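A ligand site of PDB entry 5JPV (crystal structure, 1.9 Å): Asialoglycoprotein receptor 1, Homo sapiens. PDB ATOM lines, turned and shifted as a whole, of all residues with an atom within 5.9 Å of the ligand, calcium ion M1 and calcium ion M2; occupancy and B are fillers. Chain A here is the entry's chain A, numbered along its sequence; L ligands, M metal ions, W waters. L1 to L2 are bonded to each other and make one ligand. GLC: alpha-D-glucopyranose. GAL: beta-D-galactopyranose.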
ATOM      1  N   ASP A  70      28.946   1.225 -16.295  1.00  0.00           N
ATOM      2  CA  ASP A  70      27.645   1.114 -16.983  1.00  0.00           C
ATOM      3  C   ASP A  70      26.818   2.401 -16.844  1.00  0.00           C
ATOM      4  O   ASP A  70      25.581   2.359 -16.756  1.00  0.00           O
ATOM      5  CB  ASP A  70      26.862  -0.108 -16.481  1.00  0.00           C
ATOM      6  CG  ASP A  70      26.164   0.120 -15.139  1.00  0.00           C
ATOM      7  OD1 ASP A  70      26.630   0.925 -14.310  1.00  0.00           O
ATOM      8  OD2 ASP A  70      25.122  -0.508 -14.929  1.00  0.00           O
ATOM      9  N   TRP A  75      27.347  -2.556 -19.369  1.00  0.00           N
ATOM     10  CA  TRP A  75      28.752  -2.563 -18.955  1.00  0.00           C
ATOM     11  C   TRP A  75      29.670  -2.349 -20.160  1.00  0.00           C
ATOM     12  O   TRP A  75      29.485  -3.000 -21.181  1.00  0.00           O
ATOM     13  CB  TRP A  75      29.090  -3.866 -18.235  1.00  0.00           C
ATOM     14  CG  TRP A  75      28.540  -3.897 -16.860  1.00  0.00           C
ATOM     15  CD1 TRP A  75      27.486  -4.650 -16.402  1.00  0.00           C
ATOM     16  CD2 TRP A  75      28.984  -3.118 -15.749  1.00  0.00           C
ATOM     17  NE1 TRP A  75      27.263  -4.388 -15.079  1.00  0.00           N
ATOM     18  CE2 TRP A  75      28.155  -3.445 -14.650  1.00  0.00           C
ATOM     19  CE3 TRP A  75      29.997  -2.169 -15.576  1.00  0.00           C
ATOM     20  CZ2 TRP A  75      28.321  -2.854 -13.384  1.00  0.00           C
ATOM     21  CZ3 TRP A  75      30.157  -1.584 -14.316  1.00  0.00           C
ATOM     22  CH2 TRP A  75      29.320  -1.924 -13.246  1.00  0.00           C
ATOM     23  N   ARG A  91      33.012  -9.928  -7.395  1.00  0.00           N
ATOM     24  CA  ARG A  91      32.712 -10.522  -6.081  1.00  0.00           C
ATOM     25  C   ARG A  91      31.380 -11.256  -6.177  1.00  0.00           C
ATOM     26  O   ARG A  91      30.490 -10.809  -6.921  1.00  0.00           O
ATOM     27  CB  ARG A  91      32.570  -9.437  -5.010  1.00  0.00           C
ATOM     28  CG  ARG A  91      33.839  -9.086  -4.296  1.00  0.00           C
ATOM     29  CD  ARG A  91      33.572  -8.938  -2.803  1.00  0.00           C
ATOM     30  NE  ARG A  91      34.831  -8.676  -2.098  1.00  0.00           N
ATOM     31  CZ  ARG A  91      34.971  -8.653  -0.789  1.00  0.00           C
ATOM     32  NH1 ARG A  91      33.949  -8.889   0.017  1.00  0.00           N
ATOM     33  NH2 ARG A  91      36.170  -8.394  -0.283  1.00  0.00           N
ATOM     34  N   GLU A  93      27.696 -11.963  -5.567  1.00  0.00           N
ATOM     35  CA  GLU A  93      26.612 -11.021  -5.281  1.00  0.00           C
ATOM     36  C   GLU A  93      26.819  -9.617  -5.885  1.00  0.00           C
ATOM     37  O   GLU A  93      26.032  -8.707  -5.624  1.00  0.00           O
ATOM     38  CB  GLU A  93      26.283 -10.961  -3.783  1.00  0.00           C
ATOM     39  CG  GLU A  93      25.750 -12.291  -3.228  1.00  0.00           C
ATOM     40  CD  GLU A  93      24.999 -12.127  -1.913  1.00  0.00           C
ATOM     41  OE1 GLU A  93      23.784 -12.452  -1.881  1.00  0.00           O
ATOM     42  OE2 GLU A  93      25.601 -11.655  -0.926  1.00  0.00           O
ATOM     43  N   GLN A  94      27.859  -9.474  -6.688  1.00  0.00           N
ATOM     44  CA  GLN A  94      28.117  -8.246  -7.469  1.00  0.00           C
ATOM     45  C   GLN A  94      28.117  -8.578  -8.966  1.00  0.00           C
ATOM     46  O   GLN A  94      28.359  -9.729  -9.332  1.00  0.00           O
ATOM     47  CB  GLN A  94      29.454  -7.603  -7.072  1.00  0.00           C
ATOM     48  CG  GLN A  94      29.646  -7.341  -5.556  1.00  0.00           C
ATOM     49  CD  GLN A  94      28.618  -6.389  -4.960  1.00  0.00           C
ATOM     50  OE1 GLN A  94      27.985  -5.613  -5.661  1.00  0.00           O
ATOM     51  NE2 GLN A  94      28.482  -6.436  -3.633  1.00  0.00           N
ATOM     52  N   PRO A  95      27.812  -7.590  -9.838  1.00  0.00           N
ATOM     53  CA  PRO A  95      27.348  -6.226  -9.542  1.00  0.00           C
ATOM     54  C   PRO A  95      25.883  -6.240  -9.102  1.00  0.00           C
ATOM     55  O   PRO A  95      25.133  -7.129  -9.512  1.00  0.00           O
ATOM     56  CB  PRO A  95      27.497  -5.489 -10.882  1.00  0.00           C
ATOM     57  CG  PRO A  95      27.425  -6.570 -11.927  1.00  0.00           C
ATOM     58  CD  PRO A  95      27.924  -7.838 -11.283  1.00  0.00           C
ATOM     59  N   ASP A  96      25.494  -5.293  -8.267  1.00  0.00           N
ATOM     60  CA  ASP A  96      24.127  -5.285  -7.741  1.00  0.00           C
ATOM     61  C   ASP A  96      23.401  -3.945  -7.897  1.00  0.00           C
ATOM     62  O   ASP A  96      22.266  -3.818  -7.455  1.00  0.00           O
ATOM     63  CB  ASP A  96      24.130  -5.722  -6.272  1.00  0.00           C
ATOM     64  CG  ASP A  96      24.880  -4.753  -5.358  1.00  0.00           C
ATOM     65  OD1 ASP A  96      25.544  -3.836  -5.888  1.00  0.00           O
ATOM     66  OD2 ASP A  96      24.810  -4.926  -4.122  1.00  0.00           O
ATOM     67  N   ASP A  97      24.068  -2.954  -8.494  1.00  0.00           N
ATOM     68  CA  ASP A  97      23.493  -1.605  -8.695  1.00  0.00           C
ATOM     69  C   ASP A  97      22.774  -1.070  -7.446  1.00  0.00           C
ATOM     70  O   ASP A  97      21.616  -0.642  -7.522  1.00  0.00           O
ATOM     71  CB  ASP A  97      22.533  -1.615  -9.900  1.00  0.00           C
ATOM     72  CG  ASP A  97      22.234  -0.224 -10.447  1.00  0.00           C
ATOM     73  OD1 ASP A  97      23.165   0.603 -10.605  1.00  0.00           O
ATOM     74  OD2 ASP A  97      21.045   0.031 -10.773  1.00  0.00           O
ATOM     75  N   TRP A  98      23.460  -1.095  -6.304  1.00  0.00           N
ATOM     76  CA  TRP A  98      22.814  -0.793  -5.027  1.00  0.00           C
ATOM     77  C   TRP A  98      22.404   0.679  -4.923  1.00  0.00           C
ATOM     78  O   TRP A  98      23.194   1.556  -5.224  1.00  0.00           O
ATOM     79  CB  TRP A  98      23.755  -1.195  -3.889  1.00  0.00           C
ATOM     80  CG  TRP A  98      23.235  -1.091  -2.483  1.00  0.00           C
ATOM     81  CD1 TRP A  98      22.072  -1.608  -1.978  1.00  0.00           C
ATOM     82  CD2 TRP A  98      23.893  -0.454  -1.387  1.00  0.00           C
ATOM     83  NE1 TRP A  98      21.966  -1.319  -0.637  1.00  0.00           N
ATOM     84  CE2 TRP A  98      23.073  -0.621  -0.246  1.00  0.00           C
ATOM     85  CE3 TRP A  98      25.110   0.232  -1.259  1.00  0.00           C
ATOM     86  CZ2 TRP A  98      23.416  -0.102   1.007  1.00  0.00           C
ATOM     87  CZ3 TRP A  98      25.462   0.747  -0.010  1.00  0.00           C
ATOM     88  CH2 TRP A  98      24.609   0.578   1.114  1.00  0.00           C
ATOM     89  N   GLY A 106      22.085   4.324  -8.568  1.00  0.00           N
ATOM     90  CA  GLY A 106      22.579   3.020  -8.127  1.00  0.00           C
ATOM     91  C   GLY A 106      24.101   3.059  -8.016  1.00  0.00           C
ATOM     92  O   GLY A 106      24.661   3.918  -7.318  1.00  0.00           O
ATOM     93  N   GLU A 107      24.754   2.138  -8.725  1.00  0.00           N
ATOM     94  CA  GLU A 107      26.206   2.027  -8.692  1.00  0.00           C
ATOM     95  C   GLU A 107      26.677   1.751 -10.110  1.00  0.00           C
ATOM     96  O   GLU A 107      26.238   0.786 -10.727  1.00  0.00           O
ATOM     97  CB  GLU A 107      26.640   0.923  -7.736  1.00  0.00           C
ATOM     98  CG  GLU A 107      26.424   1.273  -6.256  1.00  0.00           C
ATOM     99  CD  GLU A 107      26.828   0.143  -5.314  1.00  0.00           C
ATOM    100  OE1 GLU A 107      27.329   0.447  -4.203  1.00  0.00           O
ATOM    101  OE2 GLU A 107      26.648  -1.037  -5.683  1.00  0.00           O
ATOM    102  N   ASP A 108      27.535   2.620 -10.641  1.00  0.00           N
ATOM    103  CA  ASP A 108      27.829   2.562 -12.063  1.00  0.00           C
ATOM    104  C   ASP A 108      29.303   2.342 -12.433  1.00  0.00           C
ATOM    105  O   ASP A 108      29.623   2.273 -13.614  1.00  0.00           O
ATOM    106  CB  ASP A 108      27.298   3.820 -12.766  1.00  0.00           C
ATOM    107  CG  ASP A 108      25.763   3.899 -12.792  1.00  0.00           C
ATOM    108  OD1 ASP A 108      25.087   2.954 -12.308  1.00  0.00           O
ATOM    109  OD2 ASP A 108      25.243   4.909 -13.304  1.00  0.00           O
ATOM    110  N   HIS A 111      35.342  -1.260  -9.314  1.00  0.00           N
ATOM    111  CA  HIS A 111      36.651  -1.216  -8.670  1.00  0.00           C
ATOM    112  C   HIS A 111      37.051  -2.584  -8.138  1.00  0.00           C
ATOM    113  O   HIS A 111      36.200  -3.402  -7.819  1.00  0.00           O
ATOM    114  CB  HIS A 111      36.677  -0.180  -7.528  1.00  0.00           C
ATOM    115  CG  HIS A 111      35.747  -0.500  -6.395  1.00  0.00           C
ATOM    116  ND1 HIS A 111      36.183  -1.046  -5.196  1.00  0.00           N
ATOM    117  CD2 HIS A 111      34.407  -0.332  -6.272  1.00  0.00           C
ATOM    118  CE1 HIS A 111      35.136  -1.202  -4.392  1.00  0.00           C
ATOM    119  NE2 HIS A 111      34.056  -0.774  -5.015  1.00  0.00           N
ATOM    120  N   ASN A 119      33.672  -4.959  -7.510  1.00  0.00           N
ATOM    121  CA  ASN A 119      32.400  -4.461  -7.035  1.00  0.00           C
ATOM    122  C   ASN A 119      31.995  -3.234  -7.870  1.00  0.00           C
ATOM    123  O   ASN A 119      32.877  -2.480  -8.289  1.00  0.00           O
ATOM    124  CB  ASN A 119      32.518  -4.043  -5.574  1.00  0.00           C
ATOM    125  CG  ASN A 119      31.253  -3.415  -5.060  1.00  0.00           C
ATOM    126  OD1 ASN A 119      30.171  -3.910  -5.316  1.00  0.00           O
ATOM    127  ND2 ASN A 119      31.382  -2.293  -4.341  1.00  0.00           N
ATOM    128  N   ASP A 120      30.698  -3.052  -8.102  1.00  0.00           N
ATOM    129  CA  ASP A 120      30.200  -1.796  -8.656  1.00  0.00           C
ATOM    130  C   ASP A 120      29.903  -0.826  -7.523  1.00  0.00           C
ATOM    131  O   ASP A 120      29.346  -1.215  -6.498  1.00  0.00           O
ATOM    132  CB  ASP A 120      28.977  -1.989  -9.581  1.00  0.00           C
ATOM    133  CG  ASP A 120      27.781  -2.655  -8.898  1.00  0.00           C
ATOM    134  OD1 ASP A 120      27.951  -3.457  -7.960  1.00  0.00           O
ATOM    135  OD2 ASP A 120      26.653  -2.385  -9.340  1.00  0.00           O
ATOM    136  N   ASP A 121      30.308   0.421  -7.683  1.00  0.00           N
ATOM    137  CA  ASP A 121      30.159   1.393  -6.618  1.00  0.00           C
ATOM    138  C   ASP A 121      29.765   2.749  -7.177  1.00  0.00           C
ATOM    139  O   ASP A 121      29.679   2.930  -8.395  1.00  0.00           O
ATOM    140  CB  ASP A 121      31.452   1.505  -5.796  1.00  0.00           C
ATOM    141  CG  ASP A 121      31.197   1.833  -4.327  1.00  0.00           C
ATOM    142  OD1 ASP A 121      31.950   1.327  -3.459  1.00  0.00           O
ATOM    143  OD2 ASP A 121      30.229   2.562  -4.019  1.00  0.00           O
HETATM  144  C1  GLC L   1      31.289  -7.002   3.192  1.00  0.00           C
HETATM  145  C2  GLC L   1      30.004  -7.507   2.517  1.00  0.00           C
HETATM  146  C3  GLC L   1      29.795  -6.858   1.140  1.00  0.00           C
HETATM  147  C4  GLC L   1      29.833  -5.332   1.200  1.00  0.00           C
HETATM  148  C5  GLC L   1      31.038  -4.833   2.015  1.00  0.00           C
HETATM  149  C6  GLC L   1      30.806  -3.383   2.413  1.00  0.00           C
HETATM  150  O1  GLC L   1      32.455  -7.477   2.471  1.00  0.00           O
HETATM  151  O2  GLC L   1      30.049  -8.934   2.360  1.00  0.00           O
HETATM  152  O3  GLC L   1      28.542  -7.265   0.589  1.00  0.00           O
HETATM  153  O4  GLC L   1      29.868  -4.862  -0.170  1.00  0.00           O
HETATM  154  O5  GLC L   1      31.268  -5.549   3.273  1.00  0.00           O
HETATM  155  O6  GLC L   1      32.011  -2.658   2.198  1.00  0.00           O
HETATM  156  C1  GAL L   2      28.926  -3.809  -0.427  1.00  0.00           C
HETATM  157  C2  GAL L   2      29.401  -3.145  -1.718  1.00  0.00           C
HETATM  158  C3  GAL L   2      28.358  -2.141  -2.241  1.00  0.00           C
HETATM  159  C4  GAL L   2      26.960  -2.783  -2.312  1.00  0.00           C
HETATM  160  C5  GAL L   2      26.609  -3.384  -0.947  1.00  0.00           C
HETATM  161  C6  GAL L   2      25.236  -4.048  -0.894  1.00  0.00           C
HETATM  162  O2  GAL L   2      30.641  -2.472  -1.454  1.00  0.00           O
HETATM  163  O3  GAL L   2      28.760  -1.693  -3.549  1.00  0.00           O
HETATM  164  O4  GAL L   2      26.982  -3.797  -3.324  1.00  0.00           O
HETATM  165  O5  GAL L   2      27.608  -4.372  -0.558  1.00  0.00           O
HETATM  166  O6  GAL L   2      24.940  -4.324   0.473  1.00  0.00           O
HETATM  167 CA    CA M   1      24.639   0.412 -12.519  1.00  0.00          CA
HETATM  168 CA    CA M   2      27.839  -3.034  -5.549  1.00  0.00          CA
HETATM  169  O   HOH W   1      29.624  -8.621  -2.205  1.00  0.00           O
HETATM  170  O   HOH W   2      22.101  -4.957   0.034  1.00  0.00           O
HETATM  171  O   HOH W   3      26.156  -6.608   1.140  1.00  0.00           O
HETATM  172  O   HOH W   4      32.616  -4.676  -1.893  1.00  0.00           O
HETATM  173  O   HOH W   5      22.796  -1.293 -13.227  1.00  0.00           O
HETATM  174  O   HOH W   6      25.452  -1.796 -11.739  1.00  0.00           O
HETATM  175  O   HOH W   7      30.074   0.680  -0.741  1.00  0.00           O
HETATM  176  O   HOH W   8      22.868   1.480 -13.830  1.00  0.00           O
HETATM  177  O   HOH W   9      34.240  -1.428  -0.194  1.00  0.00           O
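O1 of GLC L1 lies within hydrogen-bond range of NH1 of Arg 91.
N of Trp 98 sits close to OE2 of Glu 107, 3.2 Å away.
The backbone NH (N) of Asp 108 is in hydrogen-bond range of the backbone carbonyl oxygen (O) of Asp 121 (3.1 Å).
OD1 of Asp 96 lies close to N of Trp 98 (3.5 Å).
N of Asp 97 is in hydrogen-bond range of OD2 of Asp 120 (2.8 Å).
O of Asn 119 is in hydrogen-bond range of N of His 111.
Merely in contact with the ligand: Trp 98.
Of the 16 residues printed, 7 come within 4 Å of the ligand.
Of the 16 residues printed, 4 come within 4 Å of calcium ion M1.
Five residues have an atom within 4 Å of calcium ion M2: Gln 94, Asp 96, Glu 107, Asn 119 and Asp 120.
Calcium ion M1 is bound by the side-chain carboxylate (OD1) of Asp 97 (2.4 Å), the backbone carbonyl oxygen (O) of Glu 107 (2.4 Å), water W8 (2.4 Å), water W6 (2.5 Å), the side-chain carboxylate (OD1) of Asp 108 (2.6 Å), water W5 (2.6 Å), the side-chain carboxylate (OD2) of Asp 70 (2.6 Å) and the side-chain carboxylate (OD1) of Asp 70 (2.7 Å).
Calcium ion M1 has eight donor atoms within binding distance.
Calcium ion M2 is bound by the side-chain carboxylate (OE2) of Glu 107 (2.3 Å), the side-chain carboxylate (OD1) of Asp 120 (2.5 Å), the side-chain carboxylate (OD1) of Asp 96 (2.5 Å), the side-chain amide oxygen (OD1) of Asn 119 (2.5 Å), an oxygen (O4) of GAL L2 (2.5 Å), the backbone carbonyl oxygen (O) of Asp 120 (2.5 Å), an oxygen (O3) of GAL L2 (2.6 Å) and the side-chain amide oxygen (OE1) of Gln 94 (2.6 Å).
Calcium ion M2 has eight donor atoms within binding distance.
Water W7 bridges an oxygen (O2) of GAL L2 and the side-chain carboxylate (OD1) of Asp 121.
Water W1 lies within hydrogen-bond range of the side-chain amide nitrogen (NE2) of Gln 94 (2.8 Å) and an oxygen (O3) of GLC L1 (3.3 Å).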
